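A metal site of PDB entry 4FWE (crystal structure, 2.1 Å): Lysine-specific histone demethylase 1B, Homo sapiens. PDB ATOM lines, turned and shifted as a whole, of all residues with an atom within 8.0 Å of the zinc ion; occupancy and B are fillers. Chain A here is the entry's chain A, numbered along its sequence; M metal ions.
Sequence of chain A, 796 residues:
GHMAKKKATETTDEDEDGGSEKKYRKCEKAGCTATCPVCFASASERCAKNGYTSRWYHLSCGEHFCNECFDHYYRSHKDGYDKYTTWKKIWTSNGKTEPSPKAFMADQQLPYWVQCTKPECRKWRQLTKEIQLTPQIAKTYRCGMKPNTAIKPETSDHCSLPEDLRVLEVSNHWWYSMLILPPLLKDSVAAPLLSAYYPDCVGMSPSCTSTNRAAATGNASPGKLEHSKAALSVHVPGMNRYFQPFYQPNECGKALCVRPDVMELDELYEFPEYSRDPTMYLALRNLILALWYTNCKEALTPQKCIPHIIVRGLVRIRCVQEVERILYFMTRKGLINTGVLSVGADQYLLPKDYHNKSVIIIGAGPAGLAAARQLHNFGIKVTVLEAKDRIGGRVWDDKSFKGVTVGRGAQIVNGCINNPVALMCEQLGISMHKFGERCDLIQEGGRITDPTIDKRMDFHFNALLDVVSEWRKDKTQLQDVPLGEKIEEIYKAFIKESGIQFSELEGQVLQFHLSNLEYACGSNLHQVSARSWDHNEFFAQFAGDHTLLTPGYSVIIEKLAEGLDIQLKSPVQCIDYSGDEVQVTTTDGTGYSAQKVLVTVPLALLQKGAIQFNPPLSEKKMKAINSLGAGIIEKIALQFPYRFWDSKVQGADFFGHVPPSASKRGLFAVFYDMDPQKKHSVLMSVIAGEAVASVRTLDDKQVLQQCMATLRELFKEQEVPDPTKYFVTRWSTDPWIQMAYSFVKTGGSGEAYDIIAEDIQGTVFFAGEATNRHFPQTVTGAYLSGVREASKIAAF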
ATOM      1  N   LYS A  26      11.437  -8.247 -21.372  1.00  0.00           N
ATOM      2  CA  LYS A  26      11.764  -8.811 -20.073  1.00  0.00           C
ATOM      3  C   LYS A  26      10.530  -8.843 -19.186  1.00  0.00           C
ATOM      4  O   LYS A  26       9.603  -8.038 -19.358  1.00  0.00           O
ATOM      5  CB  LYS A  26      12.903  -8.041 -19.397  1.00  0.00           C
ATOM      6  CG  LYS A  26      14.274  -8.482 -19.873  1.00  0.00           C
ATOM      7  N   CYS A  27      10.516  -9.796 -18.257  1.00  0.00           N
ATOM      8  CA  CYS A  27       9.379 -10.019 -17.374  1.00  0.00           C
ATOM      9  C   CYS A  27       9.057  -8.778 -16.535  1.00  0.00           C
ATOM     10  O   CYS A  27       9.941  -7.986 -16.239  1.00  0.00           O
ATOM     11  CB  CYS A  27       9.667 -11.201 -16.450  1.00  0.00           C
ATOM     12  SG  CYS A  27       8.298 -11.568 -15.332  1.00  0.00           S
ATOM     13  N   GLU A  28       7.778  -8.629 -16.165  1.00  0.00           N
ATOM     14  CA  GLU A  28       7.331  -7.549 -15.275  1.00  0.00           C
ATOM     15  C   GLU A  28       7.996  -7.629 -13.898  1.00  0.00           C
ATOM     16  O   GLU A  28       8.232  -6.605 -13.246  1.00  0.00           O
ATOM     17  CB  GLU A  28       5.795  -7.571 -15.111  1.00  0.00           C
ATOM     18  CG  GLU A  28       5.279  -8.601 -14.110  1.00  0.00           C
ATOM     19  CD  GLU A  28       3.775  -8.780 -14.125  1.00  0.00           C
ATOM     20  OE1 GLU A  28       3.335  -9.950 -14.021  1.00  0.00           O
ATOM     21  OE2 GLU A  28       3.027  -7.786 -14.225  1.00  0.00           O
ATOM     22  N   LYS A  29       8.314  -8.849 -13.459  1.00  0.00           N
ATOM     23  CA  LYS A  29       8.671  -9.123 -12.068  1.00  0.00           C
ATOM     24  C   LYS A  29      10.168  -9.021 -11.809  1.00  0.00           C
ATOM     25  O   LYS A  29      10.986  -9.396 -12.666  1.00  0.00           O
ATOM     26  CB  LYS A  29       8.175 -10.514 -11.659  1.00  0.00           C
ATOM     27  CG  LYS A  29       7.568 -10.596 -10.270  1.00  0.00           C
ATOM     28  CD  LYS A  29       6.068 -10.849 -10.345  1.00  0.00           C
ATOM     29  CE  LYS A  29       5.252  -9.567 -10.427  1.00  0.00           C
ATOM     30  NZ  LYS A  29       4.862  -9.082  -9.065  1.00  0.00           N
ATOM     31  N   ALA A  30      10.505  -8.521 -10.627  1.00  0.00           N
ATOM     32  CA  ALA A  30      11.869  -8.445 -10.143  1.00  0.00           C
ATOM     33  C   ALA A  30      12.460  -9.843  -9.944  1.00  0.00           C
ATOM     34  O   ALA A  30      11.791 -10.749  -9.452  1.00  0.00           O
ATOM     35  CB  ALA A  30      11.929  -7.654  -8.841  1.00  0.00           C
ATOM     36  N   GLY A  31      13.716 -10.005 -10.345  1.00  0.00           N
ATOM     37  CA  GLY A  31      14.449 -11.256 -10.156  1.00  0.00           C
ATOM     38  C   GLY A  31      13.881 -12.459 -10.907  1.00  0.00           C
ATOM     39  O   GLY A  31      14.177 -13.604 -10.554  1.00  0.00           O
ATOM     40  N   CYS A  32      13.067 -12.194 -11.942  1.00  0.00           N
ATOM     41  CA  CYS A  32      12.606 -13.269 -12.831  1.00  0.00           C
ATOM     42  C   CYS A  32      13.814 -13.770 -13.596  1.00  0.00           C
ATOM     43  O   CYS A  32      14.604 -12.980 -14.084  1.00  0.00           O
ATOM     44  CB  CYS A  32      11.507 -12.795 -13.793  1.00  0.00           C
ATOM     45  SG  CYS A  32      10.643 -14.151 -14.653  1.00  0.00           S
ATOM     46  N   THR A  33      13.954 -15.090 -13.694  1.00  0.00           N
ATOM     47  CA  THR A  33      15.113 -15.691 -14.337  1.00  0.00           C
ATOM     48  C   THR A  33      14.872 -16.012 -15.813  1.00  0.00           C
ATOM     49  O   THR A  33      15.728 -16.612 -16.472  1.00  0.00           O
ATOM     50  CB  THR A  33      15.529 -16.998 -13.613  1.00  0.00           C
ATOM     51  OG1 THR A  33      14.478 -17.954 -13.714  1.00  0.00           O
ATOM     52  CG2 THR A  33      15.869 -16.714 -12.137  1.00  0.00           C
ATOM     53  N   ALA A  34      13.712 -15.622 -16.338  1.00  0.00           N
ATOM     54  CA  ALA A  34      13.367 -15.918 -17.715  1.00  0.00           C
ATOM     55  C   ALA A  34      14.133 -14.995 -18.666  1.00  0.00           C
ATOM     56  O   ALA A  34      13.851 -13.797 -18.733  1.00  0.00           O
ATOM     57  CB  ALA A  34      11.868 -15.787 -17.938  1.00  0.00           C
ATOM     58  N   PRO A  37      10.869 -14.298 -22.000  1.00  0.00           N
ATOM     59  CA  PRO A  37       9.445 -14.510 -21.761  1.00  0.00           C
ATOM     60  C   PRO A  37       8.711 -14.863 -23.045  1.00  0.00           C
ATOM     61  O   PRO A  37       8.922 -14.235 -24.086  1.00  0.00           O
ATOM     62  CB  PRO A  37       8.967 -13.137 -21.270  1.00  0.00           C
ATOM     63  CG  PRO A  37      10.159 -12.511 -20.647  1.00  0.00           C
ATOM     64  CD  PRO A  37      11.354 -13.041 -21.397  1.00  0.00           C
ATOM     65  N   TRP A  56       4.792  -7.965 -19.895  1.00  0.00           N
ATOM     66  CA  TRP A  56       4.902  -9.398 -19.779  1.00  0.00           C
ATOM     67  C   TRP A  56       4.380  -9.862 -18.452  1.00  0.00           C
ATOM     68  O   TRP A  56       5.038  -9.683 -17.423  1.00  0.00           O
ATOM     69  CB  TRP A  56       6.357  -9.813 -19.959  1.00  0.00           C
ATOM     70  CG  TRP A  56       6.736 -10.054 -21.398  1.00  0.00           C
ATOM     71  CD1 TRP A  56       7.702  -9.401 -22.153  1.00  0.00           C
ATOM     72  CD2 TRP A  56       6.125 -11.030 -22.318  1.00  0.00           C
ATOM     73  NE1 TRP A  56       7.743  -9.892 -23.425  1.00  0.00           N
ATOM     74  CE2 TRP A  56       6.821 -10.870 -23.595  1.00  0.00           C
ATOM     75  CE3 TRP A  56       5.121 -11.980 -22.207  1.00  0.00           C
ATOM     76  CZ2 TRP A  56       6.516 -11.648 -24.700  1.00  0.00           C
ATOM     77  CZ3 TRP A  56       4.810 -12.756 -23.334  1.00  0.00           C
ATOM     78  CH2 TRP A  56       5.493 -12.580 -24.550  1.00  0.00           C
ATOM     79  N   TYR A  57       3.194 -10.453 -18.460  1.00  0.00           N
ATOM     80  CA  TYR A  57       2.568 -10.936 -17.239  1.00  0.00           C
ATOM     81  C   TYR A  57       3.152 -12.268 -16.750  1.00  0.00           C
ATOM     82  O   TYR A  57       3.196 -13.243 -17.505  1.00  0.00           O
ATOM     83  CB  TYR A  57       1.049 -11.027 -17.387  1.00  0.00           C
ATOM     84  CG  TYR A  57       0.386  -9.689 -17.542  1.00  0.00           C
ATOM     85  CD1 TYR A  57      -0.019  -8.948 -16.428  1.00  0.00           C
ATOM     86  CD2 TYR A  57       0.170  -9.141 -18.814  1.00  0.00           C
ATOM     87  CE1 TYR A  57      -0.622  -7.711 -16.569  1.00  0.00           C
ATOM     88  CE2 TYR A  57      -0.429  -7.910 -18.970  1.00  0.00           C
ATOM     89  CZ  TYR A  57      -0.833  -7.194 -17.840  1.00  0.00           C
ATOM     90  OH  TYR A  57      -1.422  -5.970 -17.991  1.00  0.00           O
ATOM     91  N   HIS A  58       3.573 -12.279 -15.489  1.00  0.00           N
ATOM     92  CA  HIS A  58       4.274 -13.394 -14.865  1.00  0.00           C
ATOM     93  C   HIS A  58       3.342 -14.324 -14.142  1.00  0.00           C
ATOM     94  O   HIS A  58       2.486 -13.892 -13.367  1.00  0.00           O
ATOM     95  CB  HIS A  58       5.264 -12.807 -13.875  1.00  0.00           C
ATOM     96  CG  HIS A  58       6.059 -13.826 -13.107  1.00  0.00           C
ATOM     97  ND1 HIS A  58       7.318 -14.163 -13.460  1.00  0.00           N
ATOM     98  CD2 HIS A  58       5.754 -14.569 -11.968  1.00  0.00           C
ATOM     99  CE1 HIS A  58       7.784 -15.084 -12.593  1.00  0.00           C
ATOM    100  NE2 HIS A  58       6.825 -15.338 -11.686  1.00  0.00           N
ATOM    101  N   LEU A  59       3.503 -15.627 -14.381  1.00  0.00           N
ATOM    102  CA  LEU A  59       2.852 -16.638 -13.572  1.00  0.00           C
ATOM    103  C   LEU A  59       3.926 -17.413 -12.798  1.00  0.00           C
ATOM    104  O   LEU A  59       3.860 -17.535 -11.581  1.00  0.00           O
ATOM    105  CB  LEU A  59       1.993 -17.574 -14.427  1.00  0.00           C
ATOM    106  CG  LEU A  59       0.675 -17.042 -14.995  1.00  0.00           C
ATOM    107  CD1 LEU A  59       0.033 -18.079 -15.892  1.00  0.00           C
ATOM    108  CD2 LEU A  59      -0.295 -16.650 -13.889  1.00  0.00           C
ATOM    109  N   SER A  60       4.922 -17.907 -13.528  1.00  0.00           N
ATOM    110  CA  SER A  60       6.085 -18.570 -12.954  1.00  0.00           C
ATOM    111  C   SER A  60       7.312 -18.116 -13.720  1.00  0.00           C
ATOM    112  O   SER A  60       7.198 -17.325 -14.649  1.00  0.00           O
ATOM    113  CB  SER A  60       5.927 -20.095 -13.019  1.00  0.00           C
ATOM    114  OG  SER A  60       5.809 -20.550 -14.357  1.00  0.00           O
ATOM    115  N   CYS A  61       8.484 -18.602 -13.339  1.00  0.00           N
ATOM    116  CA  CYS A  61       9.713 -18.248 -14.041  1.00  0.00           C
ATOM    117  C   CYS A  61       9.765 -18.769 -15.464  1.00  0.00           C
ATOM    118  O   CYS A  61      10.566 -18.325 -16.272  1.00  0.00           O
ATOM    119  CB  CYS A  61      10.936 -18.743 -13.263  1.00  0.00           C
ATOM    120  SG  CYS A  61      11.455 -17.599 -11.967  1.00  0.00           S
ATOM    121  N   GLY A  62       8.890 -19.719 -15.772  1.00  0.00           N
ATOM    122  CA  GLY A  62       8.873 -20.325 -17.084  1.00  0.00           C
ATOM    123  C   GLY A  62       7.589 -20.091 -17.839  1.00  0.00           C
ATOM    124  O   GLY A  62       7.384 -20.682 -18.911  1.00  0.00           O
ATOM    125  N   GLU A  63       6.729 -19.235 -17.305  1.00  0.00           N
ATOM    126  CA  GLU A  63       5.352 -19.113 -17.818  1.00  0.00           C
ATOM    127  C   GLU A  63       4.835 -17.668 -17.782  1.00  0.00           C
ATOM    128  O   GLU A  63       4.591 -17.119 -16.702  1.00  0.00           O
ATOM    129  CB  GLU A  63       4.412 -20.037 -17.036  1.00  0.00           C
ATOM    130  CG  GLU A  63       4.617 -21.520 -17.328  1.00  0.00           C
ATOM    131  CD  GLU A  63       4.049 -22.432 -16.258  1.00  0.00           C
ATOM    132  OE1 GLU A  63       4.281 -22.199 -15.054  1.00  0.00           O
ATOM    133  OE2 GLU A  63       3.383 -23.414 -16.636  1.00  0.00           O
ATOM    134  N   HIS A  64       4.689 -17.067 -18.963  1.00  0.00           N
ATOM    135  CA  HIS A  64       4.237 -15.671 -19.096  1.00  0.00           C
ATOM    136  C   HIS A  64       3.214 -15.528 -20.159  1.00  0.00           C
ATOM    137  O   HIS A  64       3.082 -16.374 -21.032  1.00  0.00           O
ATOM    138  CB  HIS A  64       5.397 -14.753 -19.430  1.00  0.00           C
ATOM    139  CG  HIS A  64       6.520 -14.805 -18.440  1.00  0.00           C
ATOM    140  ND1 HIS A  64       7.410 -15.812 -18.421  1.00  0.00           N
ATOM    141  CD2 HIS A  64       6.866 -13.936 -17.423  1.00  0.00           C
ATOM    142  CE1 HIS A  64       8.290 -15.593 -17.418  1.00  0.00           C
ATOM    143  NE2 HIS A  64       7.955 -14.437 -16.821  1.00  0.00           N
ATOM    144  N   PHE A  65       2.447 -14.445 -20.096  1.00  0.00           N
ATOM    145  CA  PHE A  65       1.565 -14.104 -21.201  1.00  0.00           C
ATOM    146  C   PHE A  65       1.639 -12.612 -21.498  1.00  0.00           C
ATOM    147  O   PHE A  65       1.987 -11.812 -20.619  1.00  0.00           O
ATOM    148  CB  PHE A  65       0.136 -14.634 -20.981  1.00  0.00           C
ATOM    149  CG  PHE A  65      -0.561 -14.067 -19.763  1.00  0.00           C
ATOM    150  CD1 PHE A  65      -0.254 -14.535 -18.487  1.00  0.00           C
ATOM    151  CD2 PHE A  65      -1.548 -13.095 -19.906  1.00  0.00           C
ATOM    152  CE1 PHE A  65      -0.901 -14.014 -17.373  1.00  0.00           C
ATOM    153  CE2 PHE A  65      -2.195 -12.573 -18.792  1.00  0.00           C
ATOM    154  CZ  PHE A  65      -1.875 -13.036 -17.515  1.00  0.00           C
ATOM    155  N   MET A 178       8.918 -17.566  -6.726  1.00  0.00           N
ATOM    156  CA  MET A 178       8.466 -16.761  -7.843  1.00  0.00           C
ATOM    157  C   MET A 178       7.135 -17.228  -8.448  1.00  0.00           C
ATOM    158  O   MET A 178       6.703 -16.710  -9.475  1.00  0.00           O
ATOM    159  CB  MET A 178       9.564 -16.668  -8.914  1.00  0.00           C
ATOM    160  CG  MET A 178      10.868 -16.047  -8.413  1.00  0.00           C
ATOM    161  SD  MET A 178      11.017 -14.241  -8.446  1.00  0.00           S
ATOM    162  CE  MET A 178       9.412 -13.650  -7.881  1.00  0.00           C
HETATM  163 ZN    ZN M   1       8.538 -13.785 -15.061  1.00  0.00          ZN
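ND1 of His 58 sits close to O of Ser 60, at 3.4 Å.
OE1 of Glu 28 lies within hydrogen-bond range of N of His 58, at 2.8 Å.
NE2 of His 58 lies within hydrogen-bond range of O of Met 178.
The backbone NH (N) of Ala 34 lies close to the side-chain sulfur (SG) of Cys 32 (3.8 Å).
N of Lys 29 sits close to SG of Cys 27 (3.3 Å).
OG of Ser 60 lies close to N of Glu 63.
The side-chain hydroxyl of Ser 60 sits close to the backbone NH of Gly 62.
Residues that only touch the zinc ion: Ser 60.
Five residues have an atom within 4 Å of the zinc ion: Cys 27, Cys 32, His 58, Ser 60 and His 64.
The nearest printed residue that does not touch the zinc ion is Cys 61 (4.7 Å).
The zinc ion is bound by a ring nitrogen (NE2) of His 64 (2.0 Å).
A ring nitrogen (ND1) of His 58 binds the zinc ion.
The zinc ion is bound by the side-chain sulfur (SG) of Cys 32 (2.2 Å).
SG of Cys 27 is bound to the zinc ion, 2.2 Å away.
The zinc ion has four donor atoms within binding distance.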
